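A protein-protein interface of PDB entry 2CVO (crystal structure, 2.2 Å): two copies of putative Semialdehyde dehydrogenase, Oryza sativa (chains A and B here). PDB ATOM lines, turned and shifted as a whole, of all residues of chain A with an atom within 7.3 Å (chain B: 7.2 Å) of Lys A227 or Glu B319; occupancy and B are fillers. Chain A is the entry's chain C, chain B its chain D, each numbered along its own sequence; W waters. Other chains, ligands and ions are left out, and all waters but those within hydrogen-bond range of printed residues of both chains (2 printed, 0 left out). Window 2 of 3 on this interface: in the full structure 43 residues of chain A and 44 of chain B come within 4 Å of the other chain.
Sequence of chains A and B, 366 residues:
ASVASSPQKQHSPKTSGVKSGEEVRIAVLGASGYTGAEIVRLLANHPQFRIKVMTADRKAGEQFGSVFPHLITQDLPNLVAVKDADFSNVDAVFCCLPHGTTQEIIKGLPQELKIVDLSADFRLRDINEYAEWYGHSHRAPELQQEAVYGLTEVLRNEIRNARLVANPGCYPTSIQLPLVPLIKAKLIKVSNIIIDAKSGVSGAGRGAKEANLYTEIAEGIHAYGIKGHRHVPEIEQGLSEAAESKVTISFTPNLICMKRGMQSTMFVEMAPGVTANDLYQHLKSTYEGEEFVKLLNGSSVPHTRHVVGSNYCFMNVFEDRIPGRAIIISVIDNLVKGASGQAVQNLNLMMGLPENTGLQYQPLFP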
ATOM      1  N   TRP A 133     -36.749  -0.059   9.240  1.00  0.00           N
ATOM      2  CA  TRP A 133     -35.331  -0.089   9.596  1.00  0.00           C
ATOM      3  C   TRP A 133     -34.958  -0.847  10.873  1.00  0.00           C
ATOM      4  O   TRP A 133     -33.783  -1.162  11.080  1.00  0.00           O
ATOM      5  CB  TRP A 133     -34.776   1.340   9.686  1.00  0.00           C
ATOM      6  CG  TRP A 133     -34.774   2.089   8.381  1.00  0.00           C
ATOM      7  CD1 TRP A 133     -35.837   2.713   7.782  1.00  0.00           C
ATOM      8  CD2 TRP A 133     -33.655   2.276   7.505  1.00  0.00           C
ATOM      9  NE1 TRP A 133     -35.447   3.277   6.588  1.00  0.00           N
ATOM     10  CE2 TRP A 133     -34.113   3.023   6.393  1.00  0.00           C
ATOM     11  CE3 TRP A 133     -32.309   1.886   7.550  1.00  0.00           C
ATOM     12  CZ2 TRP A 133     -33.270   3.389   5.336  1.00  0.00           C
ATOM     13  CZ3 TRP A 133     -31.472   2.249   6.498  1.00  0.00           C
ATOM     14  CH2 TRP A 133     -31.958   2.994   5.406  1.00  0.00           C
ATOM     15  N   TYR A 224     -18.093   0.335   6.738  1.00  0.00           N
ATOM     16  CA  TYR A 224     -19.134  -0.622   7.095  1.00  0.00           C
ATOM     17  C   TYR A 224     -20.472   0.056   6.867  1.00  0.00           C
ATOM     18  O   TYR A 224     -20.515   1.231   6.504  1.00  0.00           O
ATOM     19  CB  TYR A 224     -19.013  -1.088   8.556  1.00  0.00           C
ATOM     20  CG  TYR A 224     -19.308  -0.029   9.593  1.00  0.00           C
ATOM     21  CD1 TYR A 224     -18.320   0.858  10.015  1.00  0.00           C
ATOM     22  CD2 TYR A 224     -20.580   0.079  10.164  1.00  0.00           C
ATOM     23  CE1 TYR A 224     -18.587   1.822  10.984  1.00  0.00           C
ATOM     24  CE2 TYR A 224     -20.858   1.037  11.126  1.00  0.00           C
ATOM     25  CZ  TYR A 224     -19.852   1.906  11.533  1.00  0.00           C
ATOM     26  OH  TYR A 224     -20.108   2.849  12.504  1.00  0.00           O
ATOM     27  N   GLY A 225     -21.555  -0.690   7.063  1.00  0.00           N
ATOM     28  CA  GLY A 225     -22.887  -0.144   6.868  1.00  0.00           C
ATOM     29  C   GLY A 225     -23.035   0.614   5.562  1.00  0.00           C
ATOM     30  O   GLY A 225     -23.750   1.608   5.493  1.00  0.00           O
ATOM     31  N   ILE A 226     -22.358   0.143   4.522  1.00  0.00           N
ATOM     32  CA  ILE A 226     -22.416   0.798   3.226  1.00  0.00           C
ATOM     33  C   ILE A 226     -23.830   0.870   2.642  1.00  0.00           C
ATOM     34  O   ILE A 226     -24.575  -0.116   2.621  1.00  0.00           O
ATOM     35  CB  ILE A 226     -21.469   0.107   2.214  1.00  0.00           C
ATOM     36  CG1 ILE A 226     -20.018   0.268   2.690  1.00  0.00           C
ATOM     37  CG2 ILE A 226     -21.660   0.708   0.810  1.00  0.00           C
ATOM     38  CD1 ILE A 226     -18.995  -0.375   1.782  1.00  0.00           C
ATOM     39  N   LYS A 227     -24.174   2.071   2.182  1.00  0.00           N
ATOM     40  CA  LYS A 227     -25.462   2.387   1.578  1.00  0.00           C
ATOM     41  C   LYS A 227     -26.653   2.480   2.539  1.00  0.00           C
ATOM     42  O   LYS A 227     -27.455   3.414   2.433  1.00  0.00           O
ATOM     43  CB  LYS A 227     -25.787   1.401   0.449  1.00  0.00           C
ATOM     44  CG  LYS A 227     -27.008   1.815  -0.367  1.00  0.00           C
ATOM     45  CD  LYS A 227     -27.265   0.891  -1.544  1.00  0.00           C
ATOM     46  CE  LYS A 227     -28.458   1.375  -2.354  1.00  0.00           C
ATOM     47  NZ  LYS A 227     -28.725   0.522  -3.545  1.00  0.00           N
ATOM     48  N   GLY A 228     -26.775   1.541   3.478  1.00  0.00           N
ATOM     49  CA  GLY A 228     -27.909   1.590   4.390  1.00  0.00           C
ATOM     50  C   GLY A 228     -27.673   1.465   5.886  1.00  0.00           C
ATOM     51  O   GLY A 228     -28.098   0.490   6.502  1.00  0.00           O
ATOM     52  N   HIS A 229     -27.012   2.450   6.484  1.00  0.00           N
ATOM     53  CA  HIS A 229     -26.766   2.426   7.927  1.00  0.00           C
ATOM     54  C   HIS A 229     -28.055   2.893   8.612  1.00  0.00           C
ATOM     55  O   HIS A 229     -28.760   3.754   8.089  1.00  0.00           O
ATOM     56  CB  HIS A 229     -25.588   3.347   8.276  1.00  0.00           C
ATOM     57  CG  HIS A 229     -25.185   3.304   9.719  1.00  0.00           C
ATOM     58  ND1 HIS A 229     -25.868   3.981  10.707  1.00  0.00           N
ATOM     59  CD2 HIS A 229     -24.166   2.662  10.341  1.00  0.00           C
ATOM     60  CE1 HIS A 229     -25.288   3.761  11.873  1.00  0.00           C
ATOM     61  NE2 HIS A 229     -24.253   2.964  11.680  1.00  0.00           N
ATOM     62  N   VAL A 232     -29.091   6.617   8.763  1.00  0.00           N
ATOM     63  CA  VAL A 232     -29.432   7.366   7.553  1.00  0.00           C
ATOM     64  C   VAL A 232     -30.802   8.060   7.663  1.00  0.00           C
ATOM     65  O   VAL A 232     -30.908   9.270   7.446  1.00  0.00           O
ATOM     66  CB  VAL A 232     -29.420   6.445   6.303  1.00  0.00           C
ATOM     67  CG1 VAL A 232     -29.954   7.193   5.090  1.00  0.00           C
ATOM     68  CG2 VAL A 232     -28.001   5.966   6.029  1.00  0.00           C
ATOM     69  N   ILE A 249     -29.303  11.514   1.153  1.00  0.00           N
ATOM     70  CA  ILE A 249     -27.852  11.668   1.270  1.00  0.00           C
ATOM     71  C   ILE A 249     -27.080  10.391   0.952  1.00  0.00           C
ATOM     72  O   ILE A 249     -27.659   9.318   0.762  1.00  0.00           O
ATOM     73  CB  ILE A 249     -27.444  12.053   2.711  1.00  0.00           C
ATOM     74  CG1 ILE A 249     -27.687  10.855   3.639  1.00  0.00           C
ATOM     75  CG2 ILE A 249     -28.229  13.269   3.183  1.00  0.00           C
ATOM     76  CD1 ILE A 249     -27.344  11.103   5.091  1.00  0.00           C
ATOM     77  N   SER A 250     -25.760  10.541   0.902  1.00  0.00           N
ATOM     78  CA  SER A 250     -24.833   9.439   0.697  1.00  0.00           C
ATOM     79  C   SER A 250     -24.055   9.413   2.012  1.00  0.00           C
ATOM     80  O   SER A 250     -23.340  10.360   2.333  1.00  0.00           O
ATOM     81  CB  SER A 250     -23.877   9.730  -0.454  1.00  0.00           C
ATOM     82  OG  SER A 250     -22.881   8.722  -0.526  1.00  0.00           O
ATOM     83  N   PHE A 251     -24.204   8.341   2.779  1.00  0.00           N
ATOM     84  CA  PHE A 251     -23.536   8.238   4.074  1.00  0.00           C
ATOM     85  C   PHE A 251     -22.725   6.956   4.183  1.00  0.00           C
ATOM     86  O   PHE A 251     -23.273   5.851   4.090  1.00  0.00           O
ATOM     87  CB  PHE A 251     -24.585   8.287   5.193  1.00  0.00           C
ATOM     88  CG  PHE A 251     -24.019   8.111   6.572  1.00  0.00           C
ATOM     89  CD1 PHE A 251     -23.245   9.109   7.159  1.00  0.00           C
ATOM     90  CD2 PHE A 251     -24.248   6.935   7.283  1.00  0.00           C
ATOM     91  CE1 PHE A 251     -22.706   8.941   8.434  1.00  0.00           C
ATOM     92  CE2 PHE A 251     -23.713   6.756   8.562  1.00  0.00           C
ATOM     93  CZ  PHE A 251     -22.940   7.762   9.136  1.00  0.00           C
ATOM     94  N   THR A 252     -21.418   7.103   4.379  1.00  0.00           N
ATOM     95  CA  THR A 252     -20.538   5.946   4.499  1.00  0.00           C
ATOM     96  C   THR A 252     -19.705   6.030   5.774  1.00  0.00           C
ATOM     97  O   THR A 252     -18.796   6.861   5.889  1.00  0.00           O
ATOM     98  CB  THR A 252     -19.586   5.835   3.293  1.00  0.00           C
ATOM     99  OG1 THR A 252     -20.353   5.793   2.085  1.00  0.00           O
ATOM    100  CG2 THR A 252     -18.744   4.566   3.396  1.00  0.00           C
ATOM    101  N   PRO A 253     -20.024   5.183   6.761  1.00  0.00           N
ATOM    102  CA  PRO A 253     -19.295   5.167   8.030  1.00  0.00           C
ATOM    103  C   PRO A 253     -18.045   4.297   7.926  1.00  0.00           C
ATOM    104  O   PRO A 253     -17.986   3.383   7.104  1.00  0.00           O
ATOM    105  CB  PRO A 253     -20.325   4.604   9.001  1.00  0.00           C
ATOM    106  CG  PRO A 253     -21.036   3.595   8.149  1.00  0.00           C
ATOM    107  CD  PRO A 253     -21.235   4.344   6.840  1.00  0.00           C
ATOM    108  N   MET B 270     -21.866   7.792 -12.152  1.00  0.00           N
ATOM    109  CA  MET B 270     -21.748   6.888 -13.288  1.00  0.00           C
ATOM    110  C   MET B 270     -22.366   7.475 -14.555  1.00  0.00           C
ATOM    111  O   MET B 270     -23.202   8.367 -14.487  1.00  0.00           O
ATOM    112  CB  MET B 270     -22.417   5.559 -12.953  1.00  0.00           C
ATOM    113  CG  MET B 270     -21.865   4.925 -11.690  1.00  0.00           C
ATOM    114  SD  MET B 270     -22.628   3.354 -11.319  1.00  0.00           S
ATOM    115  CE  MET B 270     -24.141   3.909 -10.504  1.00  0.00           C
ATOM    116  N   THR B 275     -24.496   0.897 -13.998  1.00  0.00           N
ATOM    117  CA  THR B 275     -24.715   0.539 -12.594  1.00  0.00           C
ATOM    118  C   THR B 275     -23.376   0.280 -11.916  1.00  0.00           C
ATOM    119  O   THR B 275     -22.338   0.210 -12.576  1.00  0.00           O
ATOM    120  CB  THR B 275     -25.555  -0.743 -12.450  1.00  0.00           C
ATOM    121  OG1 THR B 275     -24.808  -1.857 -12.959  1.00  0.00           O
ATOM    122  CG2 THR B 275     -26.860  -0.620 -13.235  1.00  0.00           C
ATOM    123  N   ALA B 276     -23.403   0.129 -10.598  1.00  0.00           N
ATOM    124  CA  ALA B 276     -22.181  -0.132  -9.845  1.00  0.00           C
ATOM    125  C   ALA B 276     -21.612  -1.479 -10.278  1.00  0.00           C
ATOM    126  O   ALA B 276     -20.396  -1.644 -10.385  1.00  0.00           O
ATOM    127  CB  ALA B 276     -22.477  -0.133  -8.341  1.00  0.00           C
ATOM    128  N   ASN B 277     -22.494  -2.441 -10.531  1.00  0.00           N
ATOM    129  CA  ASN B 277     -22.052  -3.759 -10.972  1.00  0.00           C
ATOM    130  C   ASN B 277     -21.306  -3.652 -12.298  1.00  0.00           C
ATOM    131  O   ASN B 277     -20.329  -4.366 -12.516  1.00  0.00           O
ATOM    132  CB  ASN B 277     -23.235  -4.719 -11.137  1.00  0.00           C
ATOM    133  CG  ASN B 277     -22.794  -6.111 -11.585  1.00  0.00           C
ATOM    134  OD1 ASN B 277     -21.964  -6.750 -10.935  1.00  0.00           O
ATOM    135  ND2 ASN B 277     -23.343  -6.582 -12.698  1.00  0.00           N
ATOM    136  N   VAL B 317     -16.419  -2.160  -5.497  1.00  0.00           N
ATOM    137  CA  VAL B 317     -17.273  -1.016  -5.799  1.00  0.00           C
ATOM    138  C   VAL B 317     -18.687  -1.273  -5.299  1.00  0.00           C
ATOM    139  O   VAL B 317     -19.210  -2.380  -5.420  1.00  0.00           O
ATOM    140  CB  VAL B 317     -17.305  -0.718  -7.318  1.00  0.00           C
ATOM    141  CG1 VAL B 317     -17.588  -1.976  -8.091  1.00  0.00           C
ATOM    142  CG2 VAL B 317     -18.364   0.336  -7.619  1.00  0.00           C
ATOM    143  N   PHE B 318     -19.306  -0.243  -4.731  1.00  0.00           N
ATOM    144  CA  PHE B 318     -20.645  -0.389  -4.185  1.00  0.00           C
ATOM    145  C   PHE B 318     -21.597   0.657  -4.709  1.00  0.00           C
ATOM    146  O   PHE B 318     -21.185   1.710  -5.192  1.00  0.00           O
ATOM    147  CB  PHE B 318     -20.618  -0.288  -2.656  1.00  0.00           C
ATOM    148  CG  PHE B 318     -19.536  -1.103  -2.013  1.00  0.00           C
ATOM    149  CD1 PHE B 318     -18.227  -0.633  -1.970  1.00  0.00           C
ATOM    150  CD2 PHE B 318     -19.822  -2.349  -1.459  1.00  0.00           C
ATOM    151  CE1 PHE B 318     -17.211  -1.390  -1.382  1.00  0.00           C
ATOM    152  CE2 PHE B 318     -18.815  -3.118  -0.869  1.00  0.00           C
ATOM    153  CZ  PHE B 318     -17.505  -2.635  -0.832  1.00  0.00           C
ATOM    154  N   GLU B 319     -22.883   0.352  -4.602  1.00  0.00           N
ATOM    155  CA  GLU B 319     -23.906   1.279  -5.025  1.00  0.00           C
ATOM    156  C   GLU B 319     -23.946   2.390  -3.988  1.00  0.00           C
ATOM    157  O   GLU B 319     -23.747   2.147  -2.797  1.00  0.00           O
ATOM    158  CB  GLU B 319     -25.268   0.582  -5.081  1.00  0.00           C
ATOM    159  CG  GLU B 319     -25.443  -0.367  -6.259  1.00  0.00           C
ATOM    160  CD  GLU B 319     -26.775  -1.105  -6.228  1.00  0.00           C
ATOM    161  OE1 GLU B 319     -27.132  -1.732  -7.247  1.00  0.00           O
ATOM    162  OE2 GLU B 319     -27.465  -1.066  -5.187  1.00  0.00           O
ATOM    163  N   ASP B 320     -24.172   3.612  -4.446  1.00  0.00           N
ATOM    164  CA  ASP B 320     -24.278   4.742  -3.541  1.00  0.00           C
ATOM    165  C   ASP B 320     -25.780   4.867  -3.290  1.00  0.00           C
ATOM    166  O   ASP B 320     -26.583   4.449  -4.125  1.00  0.00           O
ATOM    167  CB  ASP B 320     -23.747   6.010  -4.212  1.00  0.00           C
ATOM    168  CG  ASP B 320     -23.744   7.207  -3.283  1.00  0.00           C
ATOM    169  OD1 ASP B 320     -22.643   7.624  -2.855  1.00  0.00           O
ATOM    170  OD2 ASP B 320     -24.841   7.730  -2.982  1.00  0.00           O
ATOM    171  N   ARG B 321     -26.165   5.419  -2.147  1.00  0.00           N
ATOM    172  CA  ARG B 321     -27.579   5.585  -1.840  1.00  0.00           C
ATOM    173  C   ARG B 321     -28.216   6.545  -2.847  1.00  0.00           C
ATOM    174  O   ARG B 321     -29.395   6.424  -3.177  1.00  0.00           O
ATOM    175  CB  ARG B 321     -27.752   6.125  -0.421  1.00  0.00           C
ATOM    176  CG  ARG B 321     -29.204   6.327  -0.002  1.00  0.00           C
ATOM    177  CD  ARG B 321     -29.284   6.803   1.442  1.00  0.00           C
ATOM    178  NE  ARG B 321     -30.645   7.124   1.857  1.00  0.00           N
ATOM    179  CZ  ARG B 321     -31.598   6.224   2.068  1.00  0.00           C
ATOM    180  NH1 ARG B 321     -31.345   4.932   1.906  1.00  0.00           N
ATOM    181  NH2 ARG B 321     -32.810   6.617   2.435  1.00  0.00           N
ATOM    182  N   ILE B 322     -27.425   7.493  -3.339  1.00  0.00           N
ATOM    183  CA  ILE B 322     -27.910   8.470  -4.305  1.00  0.00           C
ATOM    184  C   ILE B 322     -27.929   7.858  -5.693  1.00  0.00           C
ATOM    185  O   ILE B 322     -26.919   7.333  -6.166  1.00  0.00           O
ATOM    186  CB  ILE B 322     -27.018   9.725  -4.316  1.00  0.00           C
ATOM    187  CG1 ILE B 322     -27.067  10.392  -2.937  1.00  0.00           C
ATOM    188  CG2 ILE B 322     -27.485  10.702  -5.397  1.00  0.00           C
ATOM    189  CD1 ILE B 322     -26.214  11.628  -2.819  1.00  0.00           C
ATOM    190  N   ARG B 325     -25.002   7.235  -8.619  1.00  0.00           N
ATOM    191  CA  ARG B 325     -23.675   7.324  -8.012  1.00  0.00           C
ATOM    192  C   ARG B 325     -23.163   5.978  -7.526  1.00  0.00           C
ATOM    193  O   ARG B 325     -23.942   5.059  -7.260  1.00  0.00           O
ATOM    194  CB  ARG B 325     -23.683   8.316  -6.842  1.00  0.00           C
ATOM    195  CG  ARG B 325     -23.369   9.747  -7.257  1.00  0.00           C
ATOM    196  CD  ARG B 325     -23.337  10.699  -6.068  1.00  0.00           C
ATOM    197  NE  ARG B 325     -22.630  11.930  -6.411  1.00  0.00           N
ATOM    198  CZ  ARG B 325     -21.307  12.041  -6.466  1.00  0.00           C
ATOM    199  NH1 ARG B 325     -20.534  10.999  -6.195  1.00  0.00           N
ATOM    200  NH2 ARG B 325     -20.754  13.195  -6.810  1.00  0.00           N
ATOM    201  N   ALA B 326     -21.844   5.868  -7.411  1.00  0.00           N
ATOM    202  CA  ALA B 326     -21.224   4.632  -6.950  1.00  0.00           C
ATOM    203  C   ALA B 326     -20.096   4.955  -5.976  1.00  0.00           C
ATOM    204  O   ALA B 326     -19.566   6.069  -5.965  1.00  0.00           O
ATOM    205  CB  ALA B 326     -20.689   3.836  -8.140  1.00  0.00           C
ATOM    206  N   ILE B 327     -19.743   3.971  -5.158  1.00  0.00           N
ATOM    207  CA  ILE B 327     -18.692   4.121  -4.163  1.00  0.00           C
ATOM    208  C   ILE B 327     -17.592   3.099  -4.425  1.00  0.00           C
ATOM    209  O   ILE B 327     -17.853   1.899  -4.462  1.00  0.00           O
ATOM    210  CB  ILE B 327     -19.241   3.886  -2.739  1.00  0.00           C
ATOM    211  CG1 ILE B 327     -20.369   4.882  -2.447  1.00  0.00           C
ATOM    212  CG2 ILE B 327     -18.108   4.015  -1.715  1.00  0.00           C
ATOM    213  CD1 ILE B 327     -21.057   4.664  -1.120  1.00  0.00           C
HETATM  214  O   HOH W   1     -29.641   3.091   0.905  1.00  0.00           O
HETATM  215  O   HOH W   2     -24.354   6.031   0.017  1.00  0.00           O
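OE2 of Glu B319 is in salt-bridge range of NZ of Lys A227 (2.6 Å).
The side-chain hydroxyl (OG) of Ser A250 lies within hydrogen-bond range of the side-chain carboxylate (OD1) of Asp B320 (2.6 Å).
O of Ile B327 sits at hydrogen-bond distance from N of Phe B318, at 2.6 Å.
The backbone NH (N) of Ile B322 is in hydrogen-bond range of the side-chain carboxylate (OD2) of Asp B320 (2.6 Å).
The backbone NH of Asp B320 is in hydrogen-bond range of the backbone carbonyl oxygen of Arg B325 (3.2 Å).
Among the printed residues, merely in contact across the chains: Ile A226 with Phe B318 (3.8 Å), Lys A227 with Arg B321 (3.9 Å), Val A232 with Arg B321 (3.3 Å), Ile A249 with Arg B321 (3.1 Å), Ile A249 with Ile B322 (3.9 Å), Ser A250 with Ile B322 (3.8 Å) and Thr A252 with Ile B327 (3.5 Å).
Printed residues of chain B within 4 Å of Lys A227: Glu B319 (2.6 Å) and Arg B321 (3.9 Å).
Of the printed residues of chain B, Thr A252 touches Ile B327.
Asn B277 touches none of the printed residues of chain A.
Val B317 touches none of the printed residues of chain A.
Of the printed residues of chain A, Phe B318 touches Ile A226.
Glu B319 touches just one residue of chain A: Lys A227 (2.6 Å).
Of the printed residues of chain A, Ile B322 touches Ile A249 and Ser A250.
The nearest printed residue of chain B that does not touch Val A232 is Ile B322 (8.8 Å).
Of the 13 printed residues of chain A, 6 touch a printed residue of chain B.
Hydrophobic or aromatic side chains of chain A that line the printed part of chain B: Ile A226 and Val A232.
Of the 13 printed residues of chain B, 6 touch a printed residue of chain A.
Printed residues of chain B that touch a printed residue of chain A: Phe B318, Glu B319, Asp B320, Arg B321, Ile B322 and Ile B327.
Hydrophobic or aromatic side chains of chain B that line the printed part of chain A: Phe B318, Ile B322 and Ile B327.
Among the printed residues, 9 pairs touch across the chains.
Among the printed residues, Asp or Glu carboxylates within 4 Å of a Lys or Arg side-chain nitrogen of the other chain: Lys A227 with Glu B319.
No position is printed for both chains.
Water W1 bridges O of Lys A227 and NH1 of Arg B321.
Water W2 lies within hydrogen-bond range of N of Arg B321 (2.9 Å), OG of Ser A250 (3.1 Å) and OD2 of Asp B320 (3.5 Å).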
